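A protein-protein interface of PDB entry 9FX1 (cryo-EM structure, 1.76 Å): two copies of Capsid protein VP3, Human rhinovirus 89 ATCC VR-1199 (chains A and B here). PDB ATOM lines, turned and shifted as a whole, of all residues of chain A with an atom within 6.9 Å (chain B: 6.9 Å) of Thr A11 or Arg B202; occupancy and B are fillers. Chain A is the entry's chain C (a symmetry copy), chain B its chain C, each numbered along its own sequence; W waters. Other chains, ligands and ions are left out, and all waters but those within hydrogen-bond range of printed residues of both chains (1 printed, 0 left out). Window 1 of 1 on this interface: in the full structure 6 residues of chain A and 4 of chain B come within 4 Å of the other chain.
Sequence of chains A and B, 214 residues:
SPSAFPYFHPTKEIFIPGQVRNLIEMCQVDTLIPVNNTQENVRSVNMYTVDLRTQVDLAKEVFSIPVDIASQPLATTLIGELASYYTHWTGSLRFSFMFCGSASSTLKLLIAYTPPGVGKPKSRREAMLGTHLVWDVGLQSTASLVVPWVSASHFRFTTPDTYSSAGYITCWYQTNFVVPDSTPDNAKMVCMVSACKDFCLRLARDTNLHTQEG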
ATOM      1  N   TYR A   7       7.157  33.857 -20.611  1.00  0.00           N
ATOM      2  CA  TYR A   7       8.246  32.996 -20.090  1.00  0.00           C
ATOM      3  C   TYR A   7       9.236  32.574 -21.190  1.00  0.00           C
ATOM      4  O   TYR A   7      10.099  31.720 -20.988  1.00  0.00           O
ATOM      5  CB  TYR A   7       7.658  31.787 -19.350  1.00  0.00           C
ATOM      6  CG  TYR A   7       6.883  32.152 -18.097  1.00  0.00           C
ATOM      7  CD1 TYR A   7       7.556  32.262 -16.865  1.00  0.00           C
ATOM      8  CD2 TYR A   7       5.499  32.394 -18.165  1.00  0.00           C
ATOM      9  CE1 TYR A   7       6.846  32.631 -15.704  1.00  0.00           C
ATOM     10  CE2 TYR A   7       4.792  32.779 -17.009  1.00  0.00           C
ATOM     11  CZ  TYR A   7       5.463  32.898 -15.778  1.00  0.00           C
ATOM     12  OH  TYR A   7       4.777  33.274 -14.664  1.00  0.00           O
ATOM     13  N   PHE A   8       9.094  33.160 -22.374  1.00  0.00           N
ATOM     14  CA  PHE A   8       9.833  32.777 -23.565  1.00  0.00           C
ATOM     15  C   PHE A   8      11.329  33.067 -23.420  1.00  0.00           C
ATOM     16  O   PHE A   8      11.712  34.189 -23.087  1.00  0.00           O
ATOM     17  CB  PHE A   8       9.217  33.544 -24.731  1.00  0.00           C
ATOM     18  CG  PHE A   8       9.830  33.235 -26.068  1.00  0.00           C
ATOM     19  CD1 PHE A   8       9.317  32.188 -26.852  1.00  0.00           C
ATOM     20  CD2 PHE A   8      10.911  33.999 -26.533  1.00  0.00           C
ATOM     21  CE1 PHE A   8       9.891  31.900 -28.102  1.00  0.00           C
ATOM     22  CE2 PHE A   8      11.472  33.720 -27.787  1.00  0.00           C
ATOM     23  CZ  PHE A   8      10.974  32.663 -28.564  1.00  0.00           C
ATOM     24  N   HIS A   9      12.177  32.086 -23.718  1.00  0.00           N
ATOM     25  CA  HIS A   9      13.632  32.233 -23.738  1.00  0.00           C
ATOM     26  C   HIS A   9      14.127  32.263 -25.195  1.00  0.00           C
ATOM     27  O   HIS A   9      14.042  31.240 -25.876  1.00  0.00           O
ATOM     28  CB  HIS A   9      14.251  31.071 -22.953  1.00  0.00           C
ATOM     29  CG  HIS A   9      15.747  31.182 -22.846  1.00  0.00           C
ATOM     30  ND1 HIS A   9      16.434  32.056 -22.001  1.00  0.00           N
ATOM     31  CD2 HIS A   9      16.656  30.456 -23.559  1.00  0.00           C
ATOM     32  CE1 HIS A   9      17.744  31.829 -22.219  1.00  0.00           C
ATOM     33  NE2 HIS A   9      17.900  30.871 -23.145  1.00  0.00           N
ATOM     34  N   PRO A  10      14.623  33.405 -25.708  1.00  0.00           N
ATOM     35  CA  PRO A  10      15.104  33.500 -27.085  1.00  0.00           C
ATOM     36  C   PRO A  10      16.224  32.502 -27.395  1.00  0.00           C
ATOM     37  O   PRO A  10      17.024  32.159 -26.525  1.00  0.00           O
ATOM     38  CB  PRO A  10      15.587  34.943 -27.257  1.00  0.00           C
ATOM     39  CG  PRO A  10      14.776  35.718 -26.221  1.00  0.00           C
ATOM     40  CD  PRO A  10      14.654  34.716 -25.075  1.00  0.00           C
ATOM     41  N   THR A  11      16.316  32.077 -28.650  1.00  0.00           N
ATOM     42  CA  THR A  11      17.369  31.185 -29.154  1.00  0.00           C
ATOM     43  C   THR A  11      18.753  31.774 -28.862  1.00  0.00           C
ATOM     44  O   THR A  11      18.928  32.987 -29.005  1.00  0.00           O
ATOM     45  CB  THR A  11      17.188  30.973 -30.669  1.00  0.00           C
ATOM     46  OG1 THR A  11      15.928  30.392 -30.919  1.00  0.00           O
ATOM     47  CG2 THR A  11      18.249  30.049 -31.271  1.00  0.00           C
ATOM     48  N   LYS A  12      19.748  30.953 -28.494  1.00  0.00           N
ATOM     49  CA  LYS A  12      21.093  31.454 -28.168  1.00  0.00           C
ATOM     50  C   LYS A  12      21.631  32.348 -29.286  1.00  0.00           C
ATOM     51  O   LYS A  12      21.546  32.008 -30.463  1.00  0.00           O
ATOM     52  CB  LYS A  12      22.084  30.309 -27.891  1.00  0.00           C
ATOM     53  CG  LYS A  12      23.376  30.899 -27.291  1.00  0.00           C
ATOM     54  CD  LYS A  12      24.524  29.907 -27.223  1.00  0.00           C
ATOM     55  CE  LYS A  12      25.789  30.557 -26.637  1.00  0.00           C
ATOM     56  NZ  LYS A  12      26.519  31.430 -27.601  1.00  0.00           N
ATOM     57  N   GLU A  13      22.202  33.483 -28.922  1.00  0.00           N
ATOM     58  CA  GLU A  13      23.006  34.293 -29.832  1.00  0.00           C
ATOM     59  C   GLU A  13      24.344  33.581 -30.106  1.00  0.00           C
ATOM     60  O   GLU A  13      25.193  33.473 -29.217  1.00  0.00           O
ATOM     61  CB  GLU A  13      23.200  35.679 -29.206  1.00  0.00           C
ATOM     62  CG  GLU A  13      23.814  36.654 -30.211  1.00  0.00           C
ATOM     63  CD  GLU A  13      24.317  37.934 -29.541  1.00  0.00           C
ATOM     64  OE1 GLU A  13      23.695  38.440 -28.581  1.00  0.00           O
ATOM     65  OE2 GLU A  13      25.370  38.455 -29.967  1.00  0.00           O
ATOM     66  N   ILE A  14      24.525  33.046 -31.313  1.00  0.00           N
ATOM     67  CA  ILE A  14      25.815  32.480 -31.748  1.00  0.00           C
ATOM     68  C   ILE A  14      26.714  33.588 -32.292  1.00  0.00           C
ATOM     69  O   ILE A  14      26.220  34.630 -32.724  1.00  0.00           O
ATOM     70  CB  ILE A  14      25.646  31.343 -32.781  1.00  0.00           C
ATOM     71  CG1 ILE A  14      25.113  31.864 -34.136  1.00  0.00           C
ATOM     72  CG2 ILE A  14      24.820  30.203 -32.159  1.00  0.00           C
ATOM     73  CD1 ILE A  14      24.786  30.779 -35.163  1.00  0.00           C
ATOM     74  N   TYR B  85       0.627  22.378 -28.067  1.00  0.00           N
ATOM     75  CA  TYR B  85       0.402  23.640 -27.338  1.00  0.00           C
ATOM     76  C   TYR B  85       1.562  24.635 -27.463  1.00  0.00           C
ATOM     77  O   TYR B  85       1.540  25.700 -26.856  1.00  0.00           O
ATOM     78  CB  TYR B  85       0.117  23.356 -25.859  1.00  0.00           C
ATOM     79  CG  TYR B  85      -1.302  22.917 -25.619  1.00  0.00           C
ATOM     80  CD1 TYR B  85      -2.333  23.866 -25.764  1.00  0.00           C
ATOM     81  CD2 TYR B  85      -1.598  21.599 -25.235  1.00  0.00           C
ATOM     82  CE1 TYR B  85      -3.667  23.494 -25.531  1.00  0.00           C
ATOM     83  CE2 TYR B  85      -2.930  21.229 -24.980  1.00  0.00           C
ATOM     84  CZ  TYR B  85      -3.967  22.171 -25.139  1.00  0.00           C
ATOM     85  OH  TYR B  85      -5.258  21.789 -24.949  1.00  0.00           O
ATOM     86  N   TYR B  86       2.587  24.313 -28.243  1.00  0.00           N
ATOM     87  CA  TYR B  86       3.790  25.121 -28.389  1.00  0.00           C
ATOM     88  C   TYR B  86       4.200  25.208 -29.855  1.00  0.00           C
ATOM     89  O   TYR B  86       3.843  24.370 -30.675  1.00  0.00           O
ATOM     90  CB  TYR B  86       4.893  24.544 -27.501  1.00  0.00           C
ATOM     91  CG  TYR B  86       4.632  24.770 -26.022  1.00  0.00           C
ATOM     92  CD1 TYR B  86       3.880  23.853 -25.270  1.00  0.00           C
ATOM     93  CD2 TYR B  86       5.117  25.933 -25.403  1.00  0.00           C
ATOM     94  CE1 TYR B  86       3.595  24.112 -23.915  1.00  0.00           C
ATOM     95  CE2 TYR B  86       4.868  26.186 -24.044  1.00  0.00           C
ATOM     96  CZ  TYR B  86       4.093  25.278 -23.297  1.00  0.00           C
ATOM     97  OH  TYR B  86       3.830  25.526 -21.990  1.00  0.00           O
ATOM     98  N   THR B  87       4.899  26.274 -30.221  1.00  0.00           N
ATOM     99  CA  THR B  87       5.235  26.572 -31.625  1.00  0.00           C
ATOM    100  C   THR B  87       6.580  25.972 -32.028  1.00  0.00           C
ATOM    101  O   THR B  87       6.775  25.599 -33.176  1.00  0.00           O
ATOM    102  CB  THR B  87       5.248  28.094 -31.855  1.00  0.00           C
ATOM    103  OG1 THR B  87       4.077  28.695 -31.337  1.00  0.00           O
ATOM    104  CG2 THR B  87       5.329  28.468 -33.329  1.00  0.00           C
ATOM    105  N   HIS B  88       7.503  25.852 -31.079  1.00  0.00           N
ATOM    106  CA  HIS B  88       8.856  25.362 -31.318  1.00  0.00           C
ATOM    107  C   HIS B  88       9.184  24.203 -30.387  1.00  0.00           C
ATOM    108  O   HIS B  88       8.735  24.175 -29.241  1.00  0.00           O
ATOM    109  CB  HIS B  88       9.895  26.469 -31.105  1.00  0.00           C
ATOM    110  CG  HIS B  88       9.657  27.780 -31.804  1.00  0.00           C
ATOM    111  ND1 HIS B  88      10.022  29.025 -31.287  1.00  0.00           N
ATOM    112  CD2 HIS B  88       9.172  27.946 -33.065  1.00  0.00           C
ATOM    113  CE1 HIS B  88       9.712  29.920 -32.242  1.00  0.00           C
ATOM    114  NE2 HIS B  88       9.208  29.300 -33.319  1.00  0.00           N
ATOM    115  N   TRP B  89      10.039  23.308 -30.852  1.00  0.00           N
ATOM    116  CA  TRP B  89      10.594  22.238 -30.045  1.00  0.00           C
ATOM    117  C   TRP B  89      12.073  22.035 -30.357  1.00  0.00           C
ATOM    118  O   TRP B  89      12.592  22.494 -31.372  1.00  0.00           O
ATOM    119  CB  TRP B  89       9.781  20.966 -30.257  1.00  0.00           C
ATOM    120  CG  TRP B  89       9.997  20.251 -31.556  1.00  0.00           C
ATOM    121  CD1 TRP B  89       9.430  20.560 -32.743  1.00  0.00           C
ATOM    122  CD2 TRP B  89      10.823  19.076 -31.804  1.00  0.00           C
ATOM    123  NE1 TRP B  89       9.793  19.620 -33.692  1.00  0.00           N
ATOM    124  CE2 TRP B  89      10.657  18.687 -33.166  1.00  0.00           C
ATOM    125  CE3 TRP B  89      11.654  18.270 -31.000  1.00  0.00           C
ATOM    126  CZ2 TRP B  89      11.274  17.555 -33.704  1.00  0.00           C
ATOM    127  CZ3 TRP B  89      12.278  17.127 -31.533  1.00  0.00           C
ATOM    128  CH2 TRP B  89      12.092  16.769 -32.879  1.00  0.00           C
ATOM    129  N   THR B  90      12.761  21.366 -29.452  1.00  0.00           N
ATOM    130  CA  THR B  90      14.170  21.015 -29.601  1.00  0.00           C
ATOM    131  C   THR B  90      14.502  19.849 -28.686  1.00  0.00           C
ATOM    132  O   THR B  90      13.725  19.525 -27.787  1.00  0.00           O
ATOM    133  CB  THR B  90      15.061  22.225 -29.317  1.00  0.00           C
ATOM    134  OG1 THR B  90      16.413  21.942 -29.563  1.00  0.00           O
ATOM    135  CG2 THR B  90      14.960  22.678 -27.873  1.00  0.00           C
ATOM    136  N   SER B 153      19.187  24.647 -37.172  1.00  0.00           N
ATOM    137  CA  SER B 153      18.742  25.636 -36.184  1.00  0.00           C
ATOM    138  C   SER B 153      18.571  25.030 -34.784  1.00  0.00           C
ATOM    139  O   SER B 153      18.305  23.836 -34.647  1.00  0.00           O
ATOM    140  CB  SER B 153      17.438  26.271 -36.665  1.00  0.00           C
ATOM    141  OG  SER B 153      17.088  27.353 -35.827  1.00  0.00           O
ATOM    142  N   HIS B 154      18.673  25.848 -33.734  1.00  0.00           N
ATOM    143  CA  HIS B 154      18.509  25.422 -32.335  1.00  0.00           C
ATOM    144  C   HIS B 154      17.124  24.850 -32.022  1.00  0.00           C
ATOM    145  O   HIS B 154      16.996  24.043 -31.107  1.00  0.00           O
ATOM    146  CB  HIS B 154      18.782  26.612 -31.408  1.00  0.00           C
ATOM    147  CG  HIS B 154      20.245  26.937 -31.306  1.00  0.00           C
ATOM    148  ND1 HIS B 154      21.029  27.494 -32.316  1.00  0.00           N
ATOM    149  CD2 HIS B 154      21.027  26.685 -30.221  1.00  0.00           C
ATOM    150  CE1 HIS B 154      22.273  27.566 -31.812  1.00  0.00           C
ATOM    151  NE2 HIS B 154      22.298  27.092 -30.559  1.00  0.00           N
ATOM    152  N   PHE B 155      16.105  25.225 -32.789  1.00  0.00           N
ATOM    153  CA  PHE B 155      14.725  24.757 -32.642  1.00  0.00           C
ATOM    154  C   PHE B 155      14.110  24.400 -33.999  1.00  0.00           C
ATOM    155  O   PHE B 155      14.536  24.893 -35.042  1.00  0.00           O
ATOM    156  CB  PHE B 155      13.870  25.834 -31.961  1.00  0.00           C
ATOM    157  CG  PHE B 155      14.174  26.091 -30.501  1.00  0.00           C
ATOM    158  CD1 PHE B 155      15.222  26.956 -30.134  1.00  0.00           C
ATOM    159  CD2 PHE B 155      13.386  25.492 -29.502  1.00  0.00           C
ATOM    160  CE1 PHE B 155      15.504  27.191 -28.778  1.00  0.00           C
ATOM    161  CE2 PHE B 155      13.658  25.738 -28.145  1.00  0.00           C
ATOM    162  CZ  PHE B 155      14.724  26.577 -27.782  1.00  0.00           C
ATOM    163  N   CYS B 200      12.871  20.363 -25.009  1.00  0.00           N
ATOM    164  CA  CYS B 200      12.170  21.575 -24.581  1.00  0.00           C
ATOM    165  C   CYS B 200      11.125  22.015 -25.604  1.00  0.00           C
ATOM    166  O   CYS B 200      11.257  21.760 -26.801  1.00  0.00           O
ATOM    167  CB  CYS B 200      13.158  22.728 -24.347  1.00  0.00           C
ATOM    168  SG  CYS B 200      14.176  22.385 -22.901  1.00  0.00           S
ATOM    169  N   LEU B 201      10.135  22.752 -25.114  1.00  0.00           N
ATOM    170  CA  LEU B 201       9.114  23.441 -25.898  1.00  0.00           C
ATOM    171  C   LEU B 201       9.153  24.933 -25.541  1.00  0.00           C
ATOM    172  O   LEU B 201       9.446  25.288 -24.399  1.00  0.00           O
ATOM    173  CB  LEU B 201       7.731  22.845 -25.592  1.00  0.00           C
ATOM    174  CG  LEU B 201       7.567  21.337 -25.840  1.00  0.00           C
ATOM    175  CD1 LEU B 201       6.248  20.853 -25.237  1.00  0.00           C
ATOM    176  CD2 LEU B 201       7.573  21.043 -27.336  1.00  0.00           C
ATOM    177  N   ARG B 202       8.865  25.823 -26.496  1.00  0.00           N
ATOM    178  CA  ARG B 202       9.053  27.271 -26.260  1.00  0.00           C
ATOM    179  C   ARG B 202       7.787  28.116 -26.269  1.00  0.00           C
ATOM    180  O   ARG B 202       7.237  28.425 -25.220  1.00  0.00           O
ATOM    181  CB  ARG B 202      10.202  27.783 -27.136  1.00  0.00           C
ATOM    182  CG  ARG B 202      10.564  29.235 -26.807  1.00  0.00           C
ATOM    183  CD  ARG B 202      11.941  29.593 -27.371  1.00  0.00           C
ATOM    184  NE  ARG B 202      11.987  29.540 -28.846  1.00  0.00           N
ATOM    185  CZ  ARG B 202      13.012  29.921 -29.582  1.00  0.00           C
ATOM    186  NH1 ARG B 202      12.930  29.884 -30.878  1.00  0.00           N
ATOM    187  NH2 ARG B 202      14.111  30.360 -29.046  1.00  0.00           N
ATOM    188  N   LEU B 203       7.340  28.524 -27.442  1.00  0.00           N
ATOM    189  CA  LEU B 203       6.361  29.602 -27.602  1.00  0.00           C
ATOM    190  C   LEU B 203       4.923  29.066 -27.542  1.00  0.00           C
ATOM    191  O   LEU B 203       4.472  28.436 -28.497  1.00  0.00           O
ATOM    192  CB  LEU B 203       6.728  30.293 -28.924  1.00  0.00           C
ATOM    193  CG  LEU B 203       5.784  31.403 -29.415  1.00  0.00           C
ATOM    194  CD1 LEU B 203       5.703  32.548 -28.414  1.00  0.00           C
ATOM    195  CD2 LEU B 203       6.322  31.939 -30.741  1.00  0.00           C
ATOM    196  N   ALA B 204       4.231  29.263 -26.418  1.00  0.00           N
ATOM    197  CA  ALA B 204       2.892  28.717 -26.199  1.00  0.00           C
ATOM    198  C   ALA B 204       1.880  29.212 -27.251  1.00  0.00           C
ATOM    199  O   ALA B 204       1.913  30.370 -27.664  1.00  0.00           O
ATOM    200  CB  ALA B 204       2.431  29.058 -24.774  1.00  0.00           C
ATOM    201  N   ARG B 205       0.969  28.335 -27.673  1.00  0.00           N
ATOM    202  CA  ARG B 205      -0.066  28.600 -28.683  1.00  0.00           C
ATOM    203  C   ARG B 205      -1.324  27.778 -28.422  1.00  0.00           C
ATOM    204  O   ARG B 205      -1.264  26.750 -27.751  1.00  0.00           O
ATOM    205  CB  ARG B 205       0.477  28.335 -30.104  1.00  0.00           C
ATOM    206  CG  ARG B 205       0.808  26.856 -30.375  1.00  0.00           C
ATOM    207  CD  ARG B 205       1.123  26.624 -31.854  1.00  0.00           C
ATOM    208  NE  ARG B 205       1.470  25.213 -32.122  1.00  0.00           N
ATOM    209  CZ  ARG B 205       0.725  24.308 -32.725  1.00  0.00           C
ATOM    210  NH1 ARG B 205       1.246  23.184 -33.127  1.00  0.00           N
ATOM    211  NH2 ARG B 205      -0.541  24.489 -32.956  1.00  0.00           N
HETATM  212  O   HOH W   1      14.404  33.064 -30.511  1.00  0.00           O
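O of His A9 lies close to NH2 of Arg B202 (3.3 Å). The side-chain hydroxyl (OG1) of Thr A11 sits at hydrogen-bond distance from the guanidinium group (NH2) of Arg B202, 2.6 Å away.
The backbone carbonyl oxygen (O) of Leu B203 lies within hydrogen-bond range of the backbone NH (N) of Thr B87. The guanidinium group of Arg B202 sits at hydrogen-bond distance from a ring nitrogen (ND1) of His B88 (3.1 Å). O of His B154 lies within hydrogen-bond range of OG1 of Thr B90 (2.7 Å).
Among the printed residues, merely in contact across the chains: Phe A8 with Arg B202 (3.0 Å), Pro A10 with Arg B202 (3.4 Å), Thr A11 with His B154 (3.5 Å), Thr A11 with Phe B155 (3.6 Å), Phe A8 with Leu B203 (3.6 Å) and Ile A14 with His B154 (3.7 Å).
Of the printed residues of chain B, Phe A8 touches Arg B202 and Leu B203. Of chain B, only His B154, Phe B155 and Arg B202 come within 4 Å of Thr A11. Of the printed residues of chain A, Phe B155 touches Thr A11 (3.6 Å). Arg B202 touches just these residues of chain A: Phe A8 (3.0 Å), His A9 (3.1 Å), Pro A10 (3.4 Å) and Thr A11 (2.6 Å). The nearest printed residue of chain B that does not touch Phe A8 is His B88 (4.3 Å).
Of the 8 printed residues of chain A, 5 touch a printed residue of chain B. Printed residues of chain A that touch a printed residue of chain B: Phe A8, His A9, Pro A10, Thr A11 and Ile A14. Along chain A the printed residues that touch a printed residue of chain B span positions 8 to 14. Printed residues of chain B that touch a printed residue of chain A: His B154, Phe B155, Arg B202 and Leu B203. Among the printed residues, no Asp or Glu carboxylate lies within 4 Å of a Lys or Arg side-chain nitrogen of the other chain.
No position is printed for both chains.
Water W1 bridges the backbone NH (N) of Thr A11 (2.8 Å) and the guanidinium group (NH2) of Arg B202 (3.1 Å).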
